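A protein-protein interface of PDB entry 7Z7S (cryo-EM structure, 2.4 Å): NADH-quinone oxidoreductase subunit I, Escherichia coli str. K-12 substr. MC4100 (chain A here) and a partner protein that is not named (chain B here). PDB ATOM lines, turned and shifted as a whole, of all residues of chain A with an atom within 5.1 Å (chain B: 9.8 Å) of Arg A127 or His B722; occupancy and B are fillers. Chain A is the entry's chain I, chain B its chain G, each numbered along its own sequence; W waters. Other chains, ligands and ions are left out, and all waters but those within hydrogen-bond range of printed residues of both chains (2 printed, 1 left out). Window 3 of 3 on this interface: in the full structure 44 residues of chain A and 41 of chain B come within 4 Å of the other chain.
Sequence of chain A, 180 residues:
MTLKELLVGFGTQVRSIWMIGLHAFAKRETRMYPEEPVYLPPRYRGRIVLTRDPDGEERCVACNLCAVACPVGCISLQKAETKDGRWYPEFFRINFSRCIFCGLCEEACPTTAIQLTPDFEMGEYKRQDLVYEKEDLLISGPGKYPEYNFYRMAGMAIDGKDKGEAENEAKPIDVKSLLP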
ATOM      1  N   SER A  97     -16.578  11.158  35.854  1.00  0.00           N
ATOM      2  CA  SER A  97     -17.727  10.911  36.712  1.00  0.00           C
ATOM      3  C   SER A  97     -17.613   9.572  37.419  1.00  0.00           C
ATOM      4  O   SER A  97     -18.235   9.377  38.464  1.00  0.00           O
ATOM      5  CB  SER A  97     -19.022  10.983  35.903  1.00  0.00           C
ATOM      6  OG  SER A  97     -19.327   9.750  35.284  1.00  0.00           O
ATOM      7  N   TYR A 125     -21.643  20.877  35.232  1.00  0.00           N
ATOM      8  CA  TYR A 125     -23.094  20.976  35.179  1.00  0.00           C
ATOM      9  C   TYR A 125     -23.729  19.725  34.584  1.00  0.00           C
ATOM     10  O   TYR A 125     -24.629  19.139  35.186  1.00  0.00           O
ATOM     11  CB  TYR A 125     -23.495  22.217  34.386  1.00  0.00           C
ATOM     12  CG  TYR A 125     -23.077  23.500  35.050  1.00  0.00           C
ATOM     13  CD1 TYR A 125     -23.648  23.895  36.247  1.00  0.00           C
ATOM     14  CD2 TYR A 125     -22.107  24.314  34.487  1.00  0.00           C
ATOM     15  CE1 TYR A 125     -23.273  25.061  36.863  1.00  0.00           C
ATOM     16  CE2 TYR A 125     -21.722  25.485  35.098  1.00  0.00           C
ATOM     17  CZ  TYR A 125     -22.311  25.854  36.287  1.00  0.00           C
ATOM     18  OH  TYR A 125     -21.942  27.019  36.904  1.00  0.00           O
ATOM     19  N   LYS A 126     -23.272  19.306  33.412  1.00  0.00           N
ATOM     20  CA  LYS A 126     -23.724  18.076  32.781  1.00  0.00           C
ATOM     21  C   LYS A 126     -22.615  17.047  32.899  1.00  0.00           C
ATOM     22  O   LYS A 126     -21.457  17.345  32.602  1.00  0.00           O
ATOM     23  CB  LYS A 126     -24.082  18.300  31.310  1.00  0.00           C
ATOM     24  CG  LYS A 126     -24.810  19.592  31.033  1.00  0.00           C
ATOM     25  CD  LYS A 126     -26.191  19.586  31.655  1.00  0.00           C
ATOM     26  CE  LYS A 126     -27.226  20.195  30.723  1.00  0.00           C
ATOM     27  NZ  LYS A 126     -26.633  21.202  29.803  1.00  0.00           N
ATOM     28  N   ARG A 127     -22.963  15.841  33.332  1.00  0.00           N
ATOM     29  CA  ARG A 127     -21.915  14.875  33.611  1.00  0.00           C
ATOM     30  C   ARG A 127     -21.414  14.157  32.366  1.00  0.00           C
ATOM     31  O   ARG A 127     -20.427  13.424  32.457  1.00  0.00           O
ATOM     32  CB  ARG A 127     -22.386  13.882  34.673  1.00  0.00           C
ATOM     33  CG  ARG A 127     -23.070  12.655  34.188  1.00  0.00           C
ATOM     34  CD  ARG A 127     -22.827  11.543  35.181  1.00  0.00           C
ATOM     35  NE  ARG A 127     -23.886  10.546  35.162  1.00  0.00           N
ATOM     36  CZ  ARG A 127     -23.692   9.256  34.936  1.00  0.00           C
ATOM     37  NH1 ARG A 127     -22.489   8.776  34.680  1.00  0.00           N
ATOM     38  NH2 ARG A 127     -24.729   8.429  34.969  1.00  0.00           N
ATOM     39  N   GLN A 128     -22.040  14.369  31.206  1.00  0.00           N
ATOM     40  CA  GLN A 128     -21.418  13.948  29.957  1.00  0.00           C
ATOM     41  C   GLN A 128     -20.137  14.730  29.691  1.00  0.00           C
ATOM     42  O   GLN A 128     -19.212  14.207  29.064  1.00  0.00           O
ATOM     43  CB  GLN A 128     -22.404  14.104  28.798  1.00  0.00           C
ATOM     44  CG  GLN A 128     -21.916  13.579  27.452  1.00  0.00           C
ATOM     45  CD  GLN A 128     -21.764  12.072  27.420  1.00  0.00           C
ATOM     46  OE1 GLN A 128     -22.724  11.339  27.622  1.00  0.00           O
ATOM     47  NE2 GLN A 128     -20.554  11.605  27.161  1.00  0.00           N
ATOM     48  N   ASP A 129     -20.047  15.961  30.190  1.00  0.00           N
ATOM     49  CA  ASP A 129     -18.835  16.760  30.069  1.00  0.00           C
ATOM     50  C   ASP A 129     -17.717  16.296  30.990  1.00  0.00           C
ATOM     51  O   ASP A 129     -16.595  16.787  30.866  1.00  0.00           O
ATOM     52  CB  ASP A 129     -19.149  18.227  30.338  1.00  0.00           C
ATOM     53  CG  ASP A 129     -20.028  18.830  29.271  1.00  0.00           C
ATOM     54  OD1 ASP A 129     -19.565  18.957  28.121  1.00  0.00           O
ATOM     55  OD2 ASP A 129     -21.184  19.178  29.577  1.00  0.00           O
ATOM     56  N   LEU A 130     -17.991  15.371  31.903  1.00  0.00           N
ATOM     57  CA  LEU A 130     -16.949  14.754  32.704  1.00  0.00           C
ATOM     58  C   LEU A 130     -16.210  13.651  31.957  1.00  0.00           C
ATOM     59  O   LEU A 130     -15.268  13.078  32.505  1.00  0.00           O
ATOM     60  CB  LEU A 130     -17.546  14.210  34.000  1.00  0.00           C
ATOM     61  CG  LEU A 130     -17.849  15.285  35.043  1.00  0.00           C
ATOM     62  CD1 LEU A 130     -18.602  14.699  36.213  1.00  0.00           C
ATOM     63  CD2 LEU A 130     -16.571  15.945  35.500  1.00  0.00           C
ATOM     64  N   VAL A 131     -16.624  13.329  30.736  1.00  0.00           N
ATOM     65  CA  VAL A 131     -15.852  12.450  29.866  1.00  0.00           C
ATOM     66  C   VAL A 131     -14.781  13.299  29.193  1.00  0.00           C
ATOM     67  O   VAL A 131     -15.081  14.135  28.341  1.00  0.00           O
ATOM     68  CB  VAL A 131     -16.741  11.753  28.832  1.00  0.00           C
ATOM     69  CG1 VAL A 131     -15.898  10.929  27.880  1.00  0.00           C
ATOM     70  CG2 VAL A 131     -17.771  10.885  29.522  1.00  0.00           C
ATOM     71  N   TYR B 638     -23.982  -2.947  20.108  1.00  0.00           N
ATOM     72  CA  TYR B 638     -23.550  -2.439  21.405  1.00  0.00           C
ATOM     73  C   TYR B 638     -23.058  -0.999  21.307  1.00  0.00           C
ATOM     74  O   TYR B 638     -23.375  -0.173  22.166  1.00  0.00           O
ATOM     75  CB  TYR B 638     -22.466  -3.339  21.989  1.00  0.00           C
ATOM     76  CG  TYR B 638     -21.951  -2.860  23.321  1.00  0.00           C
ATOM     77  CD1 TYR B 638     -22.670  -3.081  24.481  1.00  0.00           C
ATOM     78  CD2 TYR B 638     -20.749  -2.167  23.416  1.00  0.00           C
ATOM     79  CE1 TYR B 638     -22.207  -2.637  25.699  1.00  0.00           C
ATOM     80  CE2 TYR B 638     -20.281  -1.720  24.627  1.00  0.00           C
ATOM     81  CZ  TYR B 638     -21.013  -1.959  25.765  1.00  0.00           C
ATOM     82  OH  TYR B 638     -20.541  -1.512  26.973  1.00  0.00           O
ATOM     83  N   SER B 641     -26.174   1.764  17.952  1.00  0.00           N
ATOM     84  CA  SER B 641     -27.530   1.286  18.190  1.00  0.00           C
ATOM     85  C   SER B 641     -28.374   1.270  16.922  1.00  0.00           C
ATOM     86  O   SER B 641     -29.406   0.596  16.889  1.00  0.00           O
ATOM     87  CB  SER B 641     -28.208   2.153  19.250  1.00  0.00           C
ATOM     88  OG  SER B 641     -28.056   1.592  20.540  1.00  0.00           O
ATOM     89  N   ARG B 712     -14.934  -0.852  31.032  1.00  0.00           N
ATOM     90  CA  ARG B 712     -16.377  -1.066  30.940  1.00  0.00           C
ATOM     91  C   ARG B 712     -17.163   0.230  31.115  1.00  0.00           C
ATOM     92  O   ARG B 712     -18.175   0.443  30.442  1.00  0.00           O
ATOM     93  CB  ARG B 712     -16.807  -2.097  31.981  1.00  0.00           C
ATOM     94  CG  ARG B 712     -18.298  -2.297  32.101  1.00  0.00           C
ATOM     95  CD  ARG B 712     -18.736  -3.589  31.468  1.00  0.00           C
ATOM     96  NE  ARG B 712     -19.707  -4.270  32.307  1.00  0.00           N
ATOM     97  CZ  ARG B 712     -19.812  -5.585  32.422  1.00  0.00           C
ATOM     98  NH1 ARG B 712     -19.014  -6.401  31.760  1.00  0.00           N
ATOM     99  NH2 ARG B 712     -20.754  -6.091  33.210  1.00  0.00           N
ATOM    100  N   THR B 713     -16.695   1.123  31.977  1.00  0.00           N
ATOM    101  CA  THR B 713     -17.377   2.385  32.213  1.00  0.00           C
ATOM    102  C   THR B 713     -16.800   3.535  31.400  1.00  0.00           C
ATOM    103  O   THR B 713     -17.128   4.691  31.671  1.00  0.00           O
ATOM    104  CB  THR B 713     -17.357   2.724  33.705  1.00  0.00           C
ATOM    105  OG1 THR B 713     -16.011   2.915  34.144  1.00  0.00           O
ATOM    106  CG2 THR B 713     -17.973   1.604  34.502  1.00  0.00           C
ATOM    107  N   ALA B 714     -15.960   3.252  30.411  1.00  0.00           N
ATOM    108  CA  ALA B 714     -15.419   4.289  29.542  1.00  0.00           C
ATOM    109  C   ALA B 714     -15.482   3.974  28.060  1.00  0.00           C
ATOM    110  O   ALA B 714     -15.423   4.910  27.258  1.00  0.00           O
ATOM    111  CB  ALA B 714     -13.956   4.583  29.894  1.00  0.00           C
ATOM    112  N   MET B 715     -15.585   2.704  27.667  1.00  0.00           N
ATOM    113  CA  MET B 715     -15.433   2.322  26.269  1.00  0.00           C
ATOM    114  C   MET B 715     -16.614   2.771  25.423  1.00  0.00           C
ATOM    115  O   MET B 715     -16.477   2.899  24.206  1.00  0.00           O
ATOM    116  CB  MET B 715     -15.215   0.807  26.202  1.00  0.00           C
ATOM    117  CG  MET B 715     -16.390  -0.044  26.669  1.00  0.00           C
ATOM    118  SD  MET B 715     -15.992  -1.798  26.847  1.00  0.00           S
ATOM    119  CE  MET B 715     -15.020  -2.135  25.405  1.00  0.00           C
ATOM    120  N   ARG B 716     -17.755   3.051  26.048  1.00  0.00           N
ATOM    121  CA  ARG B 716     -18.917   3.620  25.379  1.00  0.00           C
ATOM    122  C   ARG B 716     -19.241   5.022  25.878  1.00  0.00           C
ATOM    123  O   ARG B 716     -20.294   5.561  25.528  1.00  0.00           O
ATOM    124  CB  ARG B 716     -20.128   2.705  25.582  1.00  0.00           C
ATOM    125  CG  ARG B 716     -20.975   2.471  24.361  1.00  0.00           C
ATOM    126  CD  ARG B 716     -22.189   1.633  24.718  1.00  0.00           C
ATOM    127  NE  ARG B 716     -23.305   1.873  23.813  1.00  0.00           N
ATOM    128  CZ  ARG B 716     -24.186   2.854  23.958  1.00  0.00           C
ATOM    129  NH1 ARG B 716     -24.115   3.703  24.968  1.00  0.00           N
ATOM    130  NH2 ARG B 716     -25.164   2.983  23.068  1.00  0.00           N
ATOM    131  N   ALA B 717     -18.358   5.629  26.675  1.00  0.00           N
ATOM    132  CA  ALA B 717     -18.704   6.846  27.404  1.00  0.00           C
ATOM    133  C   ALA B 717     -18.800   8.065  26.498  1.00  0.00           C
ATOM    134  O   ALA B 717     -19.485   9.031  26.846  1.00  0.00           O
ATOM    135  CB  ALA B 717     -17.690   7.097  28.518  1.00  0.00           C
ATOM    136  N   ASN B 718     -18.122   8.057  25.352  1.00  0.00           N
ATOM    137  CA  ASN B 718     -18.267   9.164  24.414  1.00  0.00           C
ATOM    138  C   ASN B 718     -19.640   9.163  23.755  1.00  0.00           C
ATOM    139  O   ASN B 718     -20.148  10.226  23.384  1.00  0.00           O
ATOM    140  CB  ASN B 718     -17.168   9.109  23.354  1.00  0.00           C
ATOM    141  CG  ASN B 718     -17.251   7.870  22.496  1.00  0.00           C
ATOM    142  OD1 ASN B 718     -17.543   6.784  22.983  1.00  0.00           O
ATOM    143  ND2 ASN B 718     -16.996   8.028  21.210  1.00  0.00           N
ATOM    144  N   ILE B 719     -20.246   7.990  23.590  1.00  0.00           N
ATOM    145  CA  ILE B 719     -21.607   7.919  23.073  1.00  0.00           C
ATOM    146  C   ILE B 719     -22.597   8.361  24.140  1.00  0.00           C
ATOM    147  O   ILE B 719     -23.454   9.219  23.903  1.00  0.00           O
ATOM    148  CB  ILE B 719     -21.909   6.498  22.568  1.00  0.00           C
ATOM    149  CG1 ILE B 719     -21.112   6.211  21.297  1.00  0.00           C
ATOM    150  CG2 ILE B 719     -23.395   6.308  22.329  1.00  0.00           C
ATOM    151  CD1 ILE B 719     -20.975   4.743  20.984  1.00  0.00           C
ATOM    152  N   SER B 720     -22.480   7.796  25.335  1.00  0.00           N
ATOM    153  CA  SER B 720     -23.341   8.153  26.449  1.00  0.00           C
ATOM    154  C   SER B 720     -22.619   7.801  27.735  1.00  0.00           C
ATOM    155  O   SER B 720     -21.990   6.747  27.829  1.00  0.00           O
ATOM    156  CB  SER B 720     -24.685   7.424  26.383  1.00  0.00           C
ATOM    157  OG  SER B 720     -25.287   7.361  27.660  1.00  0.00           O
ATOM    158  N   VAL B 721     -22.725   8.684  28.727  1.00  0.00           N
ATOM    159  CA  VAL B 721     -22.109   8.430  30.020  1.00  0.00           C
ATOM    160  C   VAL B 721     -22.867   7.381  30.823  1.00  0.00           C
ATOM    161  O   VAL B 721     -22.338   6.872  31.813  1.00  0.00           O
ATOM    162  CB  VAL B 721     -21.968   9.774  30.769  1.00  0.00           C
ATOM    163  CG1 VAL B 721     -23.236  10.116  31.522  1.00  0.00           C
ATOM    164  CG2 VAL B 721     -20.761   9.761  31.685  1.00  0.00           C
ATOM    165  N   HIS B 722     -24.075   7.020  30.403  1.00  0.00           N
ATOM    166  CA  HIS B 722     -24.841   5.960  31.042  1.00  0.00           C
ATOM    167  C   HIS B 722     -24.451   4.617  30.436  1.00  0.00           C
ATOM    168  O   HIS B 722     -24.678   4.381  29.247  1.00  0.00           O
ATOM    169  CB  HIS B 722     -26.339   6.202  30.876  1.00  0.00           C
ATOM    170  CG  HIS B 722     -26.828   7.442  31.554  1.00  0.00           C
ATOM    171  ND1 HIS B 722     -27.286   7.449  32.852  1.00  0.00           N
ATOM    172  CD2 HIS B 722     -26.927   8.717  31.114  1.00  0.00           C
ATOM    173  CE1 HIS B 722     -27.648   8.673  33.183  1.00  0.00           C
ATOM    174  NE2 HIS B 722     -27.438   9.463  32.145  1.00  0.00           N
ATOM    175  N   GLU B 723     -23.874   3.747  31.252  1.00  0.00           N
ATOM    176  CA  GLU B 723     -23.502   2.417  30.788  1.00  0.00           C
ATOM    177  C   GLU B 723     -24.756   1.588  30.544  1.00  0.00           C
ATOM    178  O   GLU B 723     -25.616   1.502  31.426  1.00  0.00           O
ATOM    179  CB  GLU B 723     -22.606   1.711  31.807  1.00  0.00           C
ATOM    180  CG  GLU B 723     -21.259   2.372  32.028  1.00  0.00           C
ATOM    181  CD  GLU B 723     -21.311   3.448  33.095  1.00  0.00           C
ATOM    182  OE1 GLU B 723     -22.320   3.510  33.822  1.00  0.00           O
ATOM    183  OE2 GLU B 723     -20.352   4.240  33.201  1.00  0.00           O
ATOM    184  N   PRO B 724     -24.906   0.983  29.375  1.00  0.00           N
ATOM    185  CA  PRO B 724     -26.059   0.119  29.132  1.00  0.00           C
ATOM    186  C   PRO B 724     -25.874  -1.231  29.809  1.00  0.00           C
ATOM    187  O   PRO B 724     -24.833  -1.531  30.394  1.00  0.00           O
ATOM    188  CB  PRO B 724     -26.068  -0.024  27.611  1.00  0.00           C
ATOM    189  CG  PRO B 724     -24.644   0.082  27.240  1.00  0.00           C
ATOM    190  CD  PRO B 724     -24.003   1.031  28.214  1.00  0.00           C
ATOM    191  N   ARG B 725     -26.921  -2.042  29.735  1.00  0.00           N
ATOM    192  CA  ARG B 725     -26.775  -3.438  30.097  1.00  0.00           C
ATOM    193  C   ARG B 725     -25.835  -4.116  29.111  1.00  0.00           C
ATOM    194  O   ARG B 725     -25.759  -3.738  27.941  1.00  0.00           O
ATOM    195  CB  ARG B 725     -28.132  -4.141  30.104  1.00  0.00           C
ATOM    196  CG  ARG B 725     -28.122  -5.470  30.821  1.00  0.00           C
ATOM    197  CD  ARG B 725     -29.377  -6.269  30.595  1.00  0.00           C
ATOM    198  NE  ARG B 725     -29.355  -7.478  31.406  1.00  0.00           N
ATOM    199  CZ  ARG B 725     -30.399  -8.264  31.619  1.00  0.00           C
ATOM    200  NH1 ARG B 725     -31.578  -8.007  31.082  1.00  0.00           N
ATOM    201  NH2 ARG B 725     -30.251  -9.340  32.384  1.00  0.00           N
ATOM    202  N   GLN B 726     -25.078  -5.087  29.605  1.00  0.00           N
ATOM    203  CA  GLN B 726     -24.335  -5.946  28.704  1.00  0.00           C
ATOM    204  C   GLN B 726     -25.319  -6.654  27.781  1.00  0.00           C
ATOM    205  O   GLN B 726     -26.412  -7.029  28.221  1.00  0.00           O
ATOM    206  CB  GLN B 726     -23.504  -6.967  29.476  1.00  0.00           C
ATOM    207  CG  GLN B 726     -22.331  -6.364  30.209  1.00  0.00           C
ATOM    208  CD  GLN B 726     -21.288  -5.783  29.273  1.00  0.00           C
ATOM    209  OE1 GLN B 726     -20.519  -6.514  28.659  1.00  0.00           O
ATOM    210  NE2 GLN B 726     -21.264  -4.466  29.159  1.00  0.00           N
HETATM  211  O   HOH W   1     -23.260   5.559  35.280  1.00  0.00           O
HETATM  212  O   HOH W   2     -25.178  10.632  28.039  1.00  0.00           O
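The backbone NH (N) of His B722 sits at hydrogen-bond distance from the side-chain hydroxyl (OG) of Ser B720 (3.0 Å).
OG of Ser A97 lies within hydrogen-bond range of NH1 of Arg A127.
Ser A97 touches just one residue of chain B: Val B721.
Of chain B, only Val B721 and His B722 come within 4 Å of Arg A127.
Of the printed residues of chain B, Gln A128 touches Ala B717 (2.8 Å), Ser B720 (3.5 Å) and Val B721 (2.9 Å).
Of the printed residues of chain B, Val A131 touches Ala B717 (3.7 Å) and Val B721 (3.9 Å).
Of the printed residues of chain A, Ala B717 touches Gln A128 and Val A131.
Ile B719 touches none of the printed residues of chain A.
Printed residues of chain A within 4 Å of Ser B720: Gln A128 (3.5 Å).
Of the printed residues of chain A, Val B721 touches Ser A97, Arg A127, Gln A128 and Val A131.
His B722 touches one residue of chain A.
The nearest printed residue of chain A that does not touch Val B721 is Leu A130 (6.0 Å).
Water W2 lies within hydrogen-bond range of the side-chain amide oxygen (OE1) of Gln A128 (2.6 Å), the backbone NH (N) of Val B721 (3.2 Å) and the side-chain hydroxyl (OG) of Ser B720 (3.3 Å).
Water W1 bridges OE1 of Glu B723 (2.7 Å) and NH2 of Arg A127 (3.2 Å).
The backbone carbonyl oxygen of Ala B717 sits at hydrogen-bond distance from the side-chain amide nitrogen of Gln A128, at 2.8 Å.
The backbone carbonyl oxygen (O) of Val B721 sits at hydrogen-bond distance from the guanidinium group (NH1) of Arg A127, at 3.4 Å.
The backbone NH (N) of Val B721 lies within hydrogen-bond range of the side-chain amide oxygen (OE1) of Gln A128, at 2.9 Å.
A ring nitrogen (ND1) of His B722 sits close to the guanidinium group (NH2) of Arg A127, at 3.5 Å.
Ser A97 touches Val B721 (OG to CG2, 3.9 Å).
OE1 of Gln A128 touches CA of Ser B720, 3.5 Å away.
Ala B717 touches Val A131.
Val A131 touches Val B721.
Of the 8 printed residues of chain A, 4 touch a printed residue of chain B.
Printed residues of chain A that touch a printed residue of chain B: Ser A97, Arg A127, Gln A128 and Val A131.
Hydrophobic or aromatic side chains of chain A within 4 Å of the printed part of chain B: Val A131.
Printed residues of chain B that touch a printed residue of chain A: Ala B717, Ser B720, Val B721 and His B722.
Hydrophobic or aromatic side chains of chain B that line the printed part of chain A: Ala B717, Val B721 and His B722.
Among the printed residues, 8 pairs touch across the chains.
Among the printed residues, no Asp or Glu carboxylate lies within 4 Å of a Lys or Arg side-chain nitrogen of the other chain.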
